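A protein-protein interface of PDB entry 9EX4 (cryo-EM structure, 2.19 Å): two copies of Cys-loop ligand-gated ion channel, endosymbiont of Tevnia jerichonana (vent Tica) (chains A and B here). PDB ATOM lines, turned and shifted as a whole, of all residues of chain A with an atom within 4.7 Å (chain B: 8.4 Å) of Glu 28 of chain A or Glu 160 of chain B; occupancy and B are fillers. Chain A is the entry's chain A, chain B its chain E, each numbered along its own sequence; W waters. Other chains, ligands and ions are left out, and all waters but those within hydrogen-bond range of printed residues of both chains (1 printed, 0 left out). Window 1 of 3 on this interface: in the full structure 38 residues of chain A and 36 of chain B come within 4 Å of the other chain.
NE2 of Gln 113 of chain A lies within hydrogen-bond range of O of Leu 157 of chain B, at 3.4 Å.
The side-chain carboxylate (OE2) of Glu 160 of chain B sits close to the side-chain carboxylate (OE2) of Glu 28 of chain A, at 3.0 Å.
The backbone NH (N) of Ile 20 of chain B is in hydrogen-bond range of the backbone carbonyl oxygen (O) of Leu 157 of chain B, at 3.3 Å.
The backbone carbonyl oxygen (O) of Glu 161 of chain B lies within hydrogen-bond range of the backbone NH (N) of His 194 of chain B, at 3.1 Å.
O of Glu 28 of chain A is in hydrogen-bond range of N of Ala 114 of chain A.
The side-chain carboxylate of Glu 161 of chain B is in salt-bridge range of the guanidinium group of Arg 193 of chain B (3.5 Å).
O of Gly 158 of chain B touches OE1 of Glu 28 of chain A, at 3.9 Å.
Gln 113 of chain A touches Gln 19 of chain B.
NE2 of Gln 113 of chain A touches CA of Gly 158 of chain B, at 3.99 Å.
Arg 249 of chain A touches Glu 161 of chain B (CD to OE1, 3.8 Å).
Leu 250 of chain A touches Glu 160 of chain B.
Glu 28 of chain A touches two residues of chain B.
No residue of chain B comes within 4 Å of Ala 114 of chain A.
Of the printed residues of chain A, Gln 19 of chain B touches Gln 113 (3.5 Å).
Printed residues of chain B within 4 Å of Leu 250 of chain A: Glu 160 (3.6 Å).
Asn 24 of chain A touches none of the printed residues of chain B.
Printed residues of chain A that touch a printed residue of chain B: Glu 28, Gln 113, Arg 249 and Leu 250.
Hydrophobic or aromatic side chains of chain A within 4 Å of the printed part of chain B: Leu 250.
Along chain A the printed residues that touch a printed residue of chain B span positions 28 to 250.
Of the 15 printed residues of chain B, 5 touch a printed residue of chain A.
Printed residues of chain B that touch a printed residue of chain A: Gln 19, Leu 157, Gly 158, Glu 160 and Glu 161.
No position is printed for both chains.
Of the 7 pairs that touch across the chains among the printed residues, none has its exchanged pair printed and touching as well.
Water W1 lies within hydrogen-bond range of O of Gly 251 of chain A and ND1 of His 194 of chain B.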
ATOM      1  N   ASN A  24      35.114  40.831  31.963  1.00  0.00           N
ATOM      2  CA  ASN A  24      33.871  40.213  32.421  1.00  0.00           C
ATOM      3  C   ASN A  24      34.105  38.707  32.512  1.00  0.00           C
ATOM      4  O   ASN A  24      34.004  37.993  31.511  1.00  0.00           O
ATOM      5  CB  ASN A  24      32.719  40.550  31.477  1.00  0.00           C
ATOM      6  CG  ASN A  24      31.359  40.210  32.061  1.00  0.00           C
ATOM      7  OD1 ASN A  24      31.216  39.260  32.831  1.00  0.00           O
ATOM      8  ND2 ASN A  24      30.350  40.992  31.695  1.00  0.00           N
ATOM      9  N   GLN A  25      34.417  38.230  33.720  1.00  0.00           N
ATOM     10  CA  GLN A  25      34.652  36.804  33.916  1.00  0.00           C
ATOM     11  C   GLN A  25      33.365  35.992  33.863  1.00  0.00           C
ATOM     12  O   GLN A  25      33.416  34.798  33.548  1.00  0.00           O
ATOM     13  CB  GLN A  25      35.366  36.567  35.248  1.00  0.00           C
ATOM     14  CG  GLN A  25      34.598  37.046  36.468  1.00  0.00           C
ATOM     15  CD  GLN A  25      35.367  36.837  37.758  1.00  0.00           C
ATOM     16  OE1 GLN A  25      36.548  36.489  37.741  1.00  0.00           O
ATOM     17  NE2 GLN A  25      34.700  37.048  38.886  1.00  0.00           N
ATOM     18  N   LYS A  26      32.220  36.606  34.167  1.00  0.00           N
ATOM     19  CA  LYS A  26      30.950  35.892  34.076  1.00  0.00           C
ATOM     20  C   LYS A  26      30.637  35.503  32.636  1.00  0.00           C
ATOM     21  O   LYS A  26      30.166  34.390  32.375  1.00  0.00           O
ATOM     22  CB  LYS A  26      29.825  36.746  34.661  1.00  0.00           C
ATOM     23  CG  LYS A  26      28.470  36.059  34.693  1.00  0.00           C
ATOM     24  CD  LYS A  26      27.400  36.984  35.252  1.00  0.00           C
ATOM     25  CE  LYS A  26      26.053  36.287  35.340  1.00  0.00           C
ATOM     26  NZ  LYS A  26      26.092  35.116  36.258  1.00  0.00           N
ATOM     27  N   GLU A  27      30.889  36.407  31.690  1.00  0.00           N
ATOM     28  CA  GLU A  27      30.686  36.134  30.274  1.00  0.00           C
ATOM     29  C   GLU A  27      31.962  35.709  29.558  1.00  0.00           C
ATOM     30  O   GLU A  27      31.895  35.339  28.380  1.00  0.00           O
ATOM     31  CB  GLU A  27      30.097  37.365  29.577  1.00  0.00           C
ATOM     32  CG  GLU A  27      28.807  37.868  30.204  1.00  0.00           C
ATOM     33  CD  GLU A  27      28.285  39.126  29.539  1.00  0.00           C
ATOM     34  OE1 GLU A  27      28.835  39.516  28.488  1.00  0.00           O
ATOM     35  OE2 GLU A  27      27.326  39.725  30.069  1.00  0.00           O
ATOM     36  N   GLU A  28      33.110  35.754  30.237  1.00  0.00           N
ATOM     37  CA  GLU A  28      34.399  35.337  29.683  1.00  0.00           C
ATOM     38  C   GLU A  28      34.742  36.122  28.412  1.00  0.00           C
ATOM     39  O   GLU A  28      34.876  35.570  27.318  1.00  0.00           O
ATOM     40  CB  GLU A  28      34.421  33.826  29.427  1.00  0.00           C
ATOM     41  CG  GLU A  28      34.290  32.988  30.691  1.00  0.00           C
ATOM     42  CD  GLU A  28      34.406  31.500  30.427  1.00  0.00           C
ATOM     43  OE1 GLU A  28      34.518  31.108  29.246  1.00  0.00           O
ATOM     44  OE2 GLU A  28      34.390  30.720  31.402  1.00  0.00           O
ATOM     45  N   ASN A  29      34.886  37.435  28.582  1.00  0.00           N
ATOM     46  CA  ASN A  29      35.305  38.313  27.496  1.00  0.00           C
ATOM     47  C   ASN A  29      35.946  39.558  28.095  1.00  0.00           C
ATOM     48  O   ASN A  29      35.843  39.818  29.296  1.00  0.00           O
ATOM     49  CB  ASN A  29      34.132  38.671  26.575  1.00  0.00           C
ATOM     50  CG  ASN A  29      32.933  39.229  27.328  1.00  0.00           C
ATOM     51  OD1 ASN A  29      33.078  39.904  28.345  1.00  0.00           O
ATOM     52  ND2 ASN A  29      31.739  38.946  26.823  1.00  0.00           N
ATOM     53  N   GLN A 113      36.685  37.545  22.655  1.00  0.00           N
ATOM     54  CA  GLN A 113      36.428  36.322  23.405  1.00  0.00           C
ATOM     55  C   GLN A 113      37.673  35.874  24.164  1.00  0.00           C
ATOM     56  O   GLN A 113      38.806  36.064  23.710  1.00  0.00           O
ATOM     57  CB  GLN A 113      35.967  35.209  22.462  1.00  0.00           C
ATOM     58  CG  GLN A 113      35.477  33.947  23.160  1.00  0.00           C
ATOM     59  CD  GLN A 113      35.364  32.765  22.216  1.00  0.00           C
ATOM     60  OE1 GLN A 113      36.105  32.664  21.239  1.00  0.00           O
ATOM     61  NE2 GLN A 113      34.431  31.866  22.503  1.00  0.00           N
ATOM     62  N   ALA A 114      37.451  35.270  25.332  1.00  0.00           N
ATOM     63  CA  ALA A 114      38.522  34.723  26.168  1.00  0.00           C
ATOM     64  C   ALA A 114      38.166  33.290  26.541  1.00  0.00           C
ATOM     65  O   ALA A 114      37.668  33.026  27.645  1.00  0.00           O
ATOM     66  CB  ALA A 114      38.745  35.580  27.414  1.00  0.00           C
ATOM     67  N   PHE A 117      39.800  30.656  29.999  1.00  0.00           N
ATOM     68  CA  PHE A 117      39.606  30.854  31.431  1.00  0.00           C
ATOM     69  C   PHE A 117      39.615  29.526  32.179  1.00  0.00           C
ATOM     70  O   PHE A 117      39.128  28.506  31.683  1.00  0.00           O
ATOM     71  CB  PHE A 117      38.293  31.590  31.692  1.00  0.00           C
ATOM     72  CG  PHE A 117      38.463  33.056  31.964  1.00  0.00           C
ATOM     73  CD1 PHE A 117      38.980  33.493  33.173  1.00  0.00           C
ATOM     74  CD2 PHE A 117      38.097  33.999  31.018  1.00  0.00           C
ATOM     75  CE1 PHE A 117      39.136  34.841  33.430  1.00  0.00           C
ATOM     76  CE2 PHE A 117      38.250  35.349  31.270  1.00  0.00           C
ATOM     77  CZ  PHE A 117      38.770  35.770  32.478  1.00  0.00           C
ATOM     78  N   PHE A 119      39.016  28.479  36.401  1.00  0.00           N
ATOM     79  CA  PHE A 119      38.710  28.987  37.733  1.00  0.00           C
ATOM     80  C   PHE A 119      38.983  27.967  38.834  1.00  0.00           C
ATOM     81  O   PHE A 119      38.470  28.115  39.948  1.00  0.00           O
ATOM     82  CB  PHE A 119      37.255  29.450  37.802  1.00  0.00           C
ATOM     83  CG  PHE A 119      36.922  30.559  36.846  1.00  0.00           C
ATOM     84  CD1 PHE A 119      37.182  31.878  37.179  1.00  0.00           C
ATOM     85  CD2 PHE A 119      36.340  30.285  35.621  1.00  0.00           C
ATOM     86  CE1 PHE A 119      36.873  32.903  36.304  1.00  0.00           C
ATOM     87  CE2 PHE A 119      36.029  31.303  34.741  1.00  0.00           C
ATOM     88  CZ  PHE A 119      36.294  32.614  35.084  1.00  0.00           C
ATOM     89  N   PRO A 248      30.561  31.995  36.288  1.00  0.00           N
ATOM     90  CA  PRO A 248      29.617  31.228  35.469  1.00  0.00           C
ATOM     91  C   PRO A 248      29.243  29.922  36.154  1.00  0.00           C
ATOM     92  O   PRO A 248      29.861  29.490  37.128  1.00  0.00           O
ATOM     93  CB  PRO A 248      30.385  30.975  34.167  1.00  0.00           C
ATOM     94  CG  PRO A 248      31.488  31.987  34.162  1.00  0.00           C
ATOM     95  CD  PRO A 248      31.846  32.201  35.598  1.00  0.00           C
ATOM     96  N   ARG A 249      28.203  29.284  35.618  1.00  0.00           N
ATOM     97  CA  ARG A 249      27.719  28.012  36.155  1.00  0.00           C
ATOM     98  C   ARG A 249      28.637  26.902  35.651  1.00  0.00           C
ATOM     99  O   ARG A 249      28.333  26.165  34.709  1.00  0.00           O
ATOM    100  CB  ARG A 249      26.263  27.783  35.767  1.00  0.00           C
ATOM    101  CG  ARG A 249      25.330  28.873  36.275  1.00  0.00           C
ATOM    102  CD  ARG A 249      23.867  28.538  36.043  1.00  0.00           C
ATOM    103  NE  ARG A 249      22.990  29.550  36.617  1.00  0.00           N
ATOM    104  CZ  ARG A 249      21.666  29.474  36.641  1.00  0.00           C
ATOM    105  NH1 ARG A 249      21.024  28.438  36.126  1.00  0.00           N
ATOM    106  NH2 ARG A 249      20.969  30.462  37.195  1.00  0.00           N
ATOM    107  N   LEU A 250      29.791  26.790  36.306  1.00  0.00           N
ATOM    108  CA  LEU A 250      30.828  25.859  35.893  1.00  0.00           C
ATOM    109  C   LEU A 250      30.437  24.419  36.216  1.00  0.00           C
ATOM    110  O   LEU A 250      29.605  24.148  37.087  1.00  0.00           O
ATOM    111  CB  LEU A 250      32.152  26.199  36.576  1.00  0.00           C
ATOM    112  CG  LEU A 250      32.742  27.582  36.293  1.00  0.00           C
ATOM    113  CD1 LEU A 250      33.942  27.840  37.188  1.00  0.00           C
ATOM    114  CD2 LEU A 250      33.125  27.709  34.829  1.00  0.00           C
ATOM    115  N   GLY A 251      31.056  23.492  35.496  1.00  0.00           N
ATOM    116  CA  GLY A 251      30.874  22.071  35.694  1.00  0.00           C
ATOM    117  C   GLY A 251      31.844  21.418  36.655  1.00  0.00           C
ATOM    118  O   GLY A 251      31.838  20.187  36.772  1.00  0.00           O
ATOM    119  N   GLN B  19      31.333  30.674  17.443  1.00  0.00           N
ATOM    120  CA  GLN B  19      31.217  30.966  18.863  1.00  0.00           C
ATOM    121  C   GLN B  19      29.758  30.924  19.294  1.00  0.00           C
ATOM    122  O   GLN B  19      28.853  31.212  18.508  1.00  0.00           O
ATOM    123  CB  GLN B  19      31.803  32.346  19.211  1.00  0.00           C
ATOM    124  CG  GLN B  19      33.229  32.576  18.743  1.00  0.00           C
ATOM    125  CD  GLN B  19      33.735  33.964  19.092  1.00  0.00           C
ATOM    126  OE1 GLN B  19      33.285  34.574  20.061  1.00  0.00           O
ATOM    127  NE2 GLN B  19      34.669  34.470  18.298  1.00  0.00           N
ATOM    128  N   ILE B  20      29.543  30.554  20.553  1.00  0.00           N
ATOM    129  CA  ILE B  20      28.243  30.666  21.208  1.00  0.00           C
ATOM    130  C   ILE B  20      28.432  31.661  22.346  1.00  0.00           C
ATOM    131  O   ILE B  20      28.998  31.325  23.393  1.00  0.00           O
ATOM    132  CB  ILE B  20      27.724  29.319  21.720  1.00  0.00           C
ATOM    133  CG1 ILE B  20      27.510  28.351  20.554  1.00  0.00           C
ATOM    134  CG2 ILE B  20      26.429  29.509  22.498  1.00  0.00           C
ATOM    135  CD1 ILE B  20      26.949  27.008  20.971  1.00  0.00           C
ATOM    136  N   THR B  21      27.962  32.893  22.147  1.00  0.00           N
ATOM    137  CA  THR B  21      28.221  33.965  23.100  1.00  0.00           C
ATOM    138  C   THR B  21      27.247  33.981  24.271  1.00  0.00           C
ATOM    139  O   THR B  21      27.492  34.703  25.244  1.00  0.00           O
ATOM    140  CB  THR B  21      28.183  35.322  22.392  1.00  0.00           C
ATOM    141  OG1 THR B  21      26.888  35.527  21.814  1.00  0.00           O
ATOM    142  CG2 THR B  21      29.235  35.377  21.294  1.00  0.00           C
ATOM    143  N   ILE B  23      23.273  31.920  25.996  1.00  0.00           N
ATOM    144  CA  ILE B  23      21.939  31.344  25.876  1.00  0.00           C
ATOM    145  C   ILE B  23      21.074  31.949  26.972  1.00  0.00           C
ATOM    146  O   ILE B  23      21.400  31.835  28.158  1.00  0.00           O
ATOM    147  CB  ILE B  23      21.958  29.810  25.986  1.00  0.00           C
ATOM    148  CG1 ILE B  23      22.814  29.205  24.870  1.00  0.00           C
ATOM    149  CG2 ILE B  23      20.543  29.254  25.940  1.00  0.00           C
ATOM    150  CD1 ILE B  23      22.899  27.696  24.914  1.00  0.00           C
ATOM    151  N   LEU B 157      33.935  26.678  21.266  1.00  0.00           N
ATOM    152  CA  LEU B 157      32.652  27.366  21.361  1.00  0.00           C
ATOM    153  C   LEU B 157      32.617  28.336  22.537  1.00  0.00           C
ATOM    154  O   LEU B 157      32.014  29.411  22.438  1.00  0.00           O
ATOM    155  CB  LEU B 157      31.517  26.349  21.471  1.00  0.00           C
ATOM    156  CG  LEU B 157      31.304  25.436  20.263  1.00  0.00           C
ATOM    157  CD1 LEU B 157      30.134  24.491  20.499  1.00  0.00           C
ATOM    158  CD2 LEU B 157      31.090  26.258  19.002  1.00  0.00           C
ATOM    159  N   GLY B 158      33.251  27.978  23.651  1.00  0.00           N
ATOM    160  CA  GLY B 158      33.291  28.830  24.819  1.00  0.00           C
ATOM    161  C   GLY B 158      32.125  28.689  25.774  1.00  0.00           C
ATOM    162  O   GLY B 158      32.069  29.425  26.767  1.00  0.00           O
ATOM    163  N   GLU B 159      31.194  27.774  25.512  1.00  0.00           N
ATOM    164  CA  GLU B 159      30.065  27.563  26.407  1.00  0.00           C
ATOM    165  C   GLU B 159      30.489  26.688  27.582  1.00  0.00           C
ATOM    166  O   GLU B 159      31.171  25.674  27.399  1.00  0.00           O
ATOM    167  CB  GLU B 159      28.900  26.921  25.656  1.00  0.00           C
ATOM    168  CG  GLU B 159      27.667  26.667  26.510  1.00  0.00           C
ATOM    169  CD  GLU B 159      27.023  27.949  27.009  1.00  0.00           C
ATOM    170  OE1 GLU B 159      27.173  28.994  26.343  1.00  0.00           O
ATOM    171  OE2 GLU B 159      26.368  27.908  28.071  1.00  0.00           O
ATOM    172  N   GLU B 160      30.082  27.082  28.788  1.00  0.00           N
ATOM    173  CA  GLU B 160      30.478  26.381  30.004  1.00  0.00           C
ATOM    174  C   GLU B 160      29.402  25.457  30.553  1.00  0.00           C
ATOM    175  O   GLU B 160      29.734  24.434  31.162  1.00  0.00           O
ATOM    176  CB  GLU B 160      30.868  27.386  31.092  1.00  0.00           C
ATOM    177  CG  GLU B 160      32.118  28.196  30.784  1.00  0.00           C
ATOM    178  CD  GLU B 160      33.394  27.396  30.955  1.00  0.00           C
ATOM    179  OE1 GLU B 160      33.328  26.268  31.489  1.00  0.00           O
ATOM    180  OE2 GLU B 160      34.466  27.895  30.555  1.00  0.00           O
ATOM    181  N   GLU B 161      28.125  25.784  30.360  1.00  0.00           N
ATOM    182  CA  GLU B 161      27.037  25.017  30.956  1.00  0.00           C
ATOM    183  C   GLU B 161      26.448  23.965  30.026  1.00  0.00           C
ATOM    184  O   GLU B 161      26.060  22.891  30.496  1.00  0.00           O
ATOM    185  CB  GLU B 161      25.919  25.960  31.418  1.00  0.00           C
ATOM    186  CG  GLU B 161      24.809  25.278  32.205  1.00  0.00           C
ATOM    187  CD  GLU B 161      23.752  26.250  32.687  1.00  0.00           C
ATOM    188  OE1 GLU B 161      23.886  27.461  32.416  1.00  0.00           O
ATOM    189  OE2 GLU B 161      22.785  25.802  33.339  1.00  0.00           O
ATOM    190  N   TRP B 162      26.378  24.234  28.726  1.00  0.00           N
ATOM    191  CA  TRP B 162      25.727  23.341  27.779  1.00  0.00           C
ATOM    192  C   TRP B 162      26.750  22.500  27.026  1.00  0.00           C
ATOM    193  O   TRP B 162      27.853  22.958  26.717  1.00  0.00           O
ATOM    194  CB  TRP B 162      24.873  24.132  26.787  1.00  0.00           C
ATOM    195  CG  TRP B 162      23.742  24.878  27.431  1.00  0.00           C
ATOM    196  CD1 TRP B 162      23.793  26.120  27.994  1.00  0.00           C
ATOM    197  CD2 TRP B 162      22.390  24.426  27.580  1.00  0.00           C
ATOM    198  NE1 TRP B 162      22.558  26.470  28.483  1.00  0.00           N
ATOM    199  CE2 TRP B 162      21.679  25.447  28.242  1.00  0.00           C
ATOM    200  CE3 TRP B 162      21.711  23.259  27.217  1.00  0.00           C
ATOM    201  CZ2 TRP B 162      20.324  25.337  28.547  1.00  0.00           C
ATOM    202  CZ3 TRP B 162      20.367  23.150  27.521  1.00  0.00           C
ATOM    203  CH2 TRP B 162      19.688  24.184  28.180  1.00  0.00           C
ATOM    204  N   ILE B 163      26.371  21.255  26.736  1.00  0.00           N
ATOM    205  CA  ILE B 163      27.206  20.315  25.996  1.00  0.00           C
ATOM    206  C   ILE B 163      26.450  19.888  24.747  1.00  0.00           C
ATOM    207  O   ILE B 163      25.315  19.406  24.838  1.00  0.00           O
ATOM    208  CB  ILE B 163      27.577  19.084  26.846  1.00  0.00           C
ATOM    209  CG1 ILE B 163      28.082  19.503  28.228  1.00  0.00           C
ATOM    210  CG2 ILE B 163      28.618  18.239  26.128  1.00  0.00           C
ATOM    211  CD1 ILE B 163      27.030  19.409  29.317  1.00  0.00           C
ATOM    212  N   GLU B 192      22.581  19.533  26.156  1.00  0.00           N
ATOM    213  CA  GLU B 192      22.110  19.205  27.495  1.00  0.00           C
ATOM    214  C   GLU B 192      22.871  20.058  28.507  1.00  0.00           C
ATOM    215  O   GLU B 192      23.721  20.877  28.147  1.00  0.00           O
ATOM    216  CB  GLU B 192      22.265  17.707  27.792  1.00  0.00           C
ATOM    217  CG  GLU B 192      23.690  17.191  27.735  1.00  0.00           C
ATOM    218  CD  GLU B 192      23.769  15.694  27.959  1.00  0.00           C
ATOM    219  OE1 GLU B 192      22.711  15.030  27.923  1.00  0.00           O
ATOM    220  OE2 GLU B 192      24.887  15.180  28.173  1.00  0.00           O
ATOM    221  N   ARG B 193      22.568  19.860  29.788  1.00  0.00           N
ATOM    222  CA  ARG B 193      22.991  20.768  30.843  1.00  0.00           C
ATOM    223  C   ARG B 193      23.906  20.069  31.843  1.00  0.00           C
ATOM    224  O   ARG B 193      23.774  18.868  32.100  1.00  0.00           O
ATOM    225  CB  ARG B 193      21.772  21.344  31.573  1.00  0.00           C
ATOM    226  CG  ARG B 193      22.000  22.689  32.229  1.00  0.00           C
ATOM    227  CD  ARG B 193      20.785  23.099  33.043  1.00  0.00           C
ATOM    228  NE  ARG B 193      19.565  23.131  32.246  1.00  0.00           N
ATOM    229  CZ  ARG B 193      19.014  24.236  31.761  1.00  0.00           C
ATOM    230  NH1 ARG B 193      19.553  25.425  31.971  1.00  0.00           N
ATOM    231  NH2 ARG B 193      17.895  24.144  31.050  1.00  0.00           N
ATOM    232  N   HIS B 194      24.841  20.838  32.401  1.00  0.00           N
ATOM    233  CA  HIS B 194      25.661  20.368  33.511  1.00  0.00           C
ATOM    234  C   HIS B 194      24.889  20.482  34.819  1.00  0.00           C
ATOM    235  O   HIS B 194      24.107  21.416  35.016  1.00  0.00           O
ATOM    236  CB  HIS B 194      26.958  21.173  33.606  1.00  0.00           C
ATOM    237  CG  HIS B 194      28.048  20.684  32.704  1.00  0.00           C
ATOM    238  ND1 HIS B 194      28.588  19.420  32.808  1.00  0.00           N
ATOM    239  CD2 HIS B 194      28.710  21.294  31.692  1.00  0.00           C
ATOM    240  CE1 HIS B 194      29.530  19.270  31.893  1.00  0.00           C
ATOM    241  NE2 HIS B 194      29.624  20.392  31.203  1.00  0.00           N
ATOM    242  N   LEU B 195      25.114  19.524  35.718  1.00  0.00           N
ATOM    243  CA  LEU B 195      24.390  19.454  36.981  1.00  0.00           C
ATOM    244  C   LEU B 195      25.225  19.861  38.188  1.00  0.00           C
ATOM    245  O   LEU B 195      24.701  19.865  39.308  1.00  0.00           O
ATOM    246  CB  LEU B 195      23.843  18.038  37.193  1.00  0.00           C
ATOM    247  CG  LEU B 195      22.931  17.498  36.089  1.00  0.00           C
ATOM    248  CD1 LEU B 195      22.489  16.079  36.405  1.00  0.00           C
ATOM    249  CD2 LEU B 195      21.729  18.408  35.895  1.00  0.00           C
HETATM  250  O   HOH W   1      29.023  18.795  36.037  1.00  0.00           O
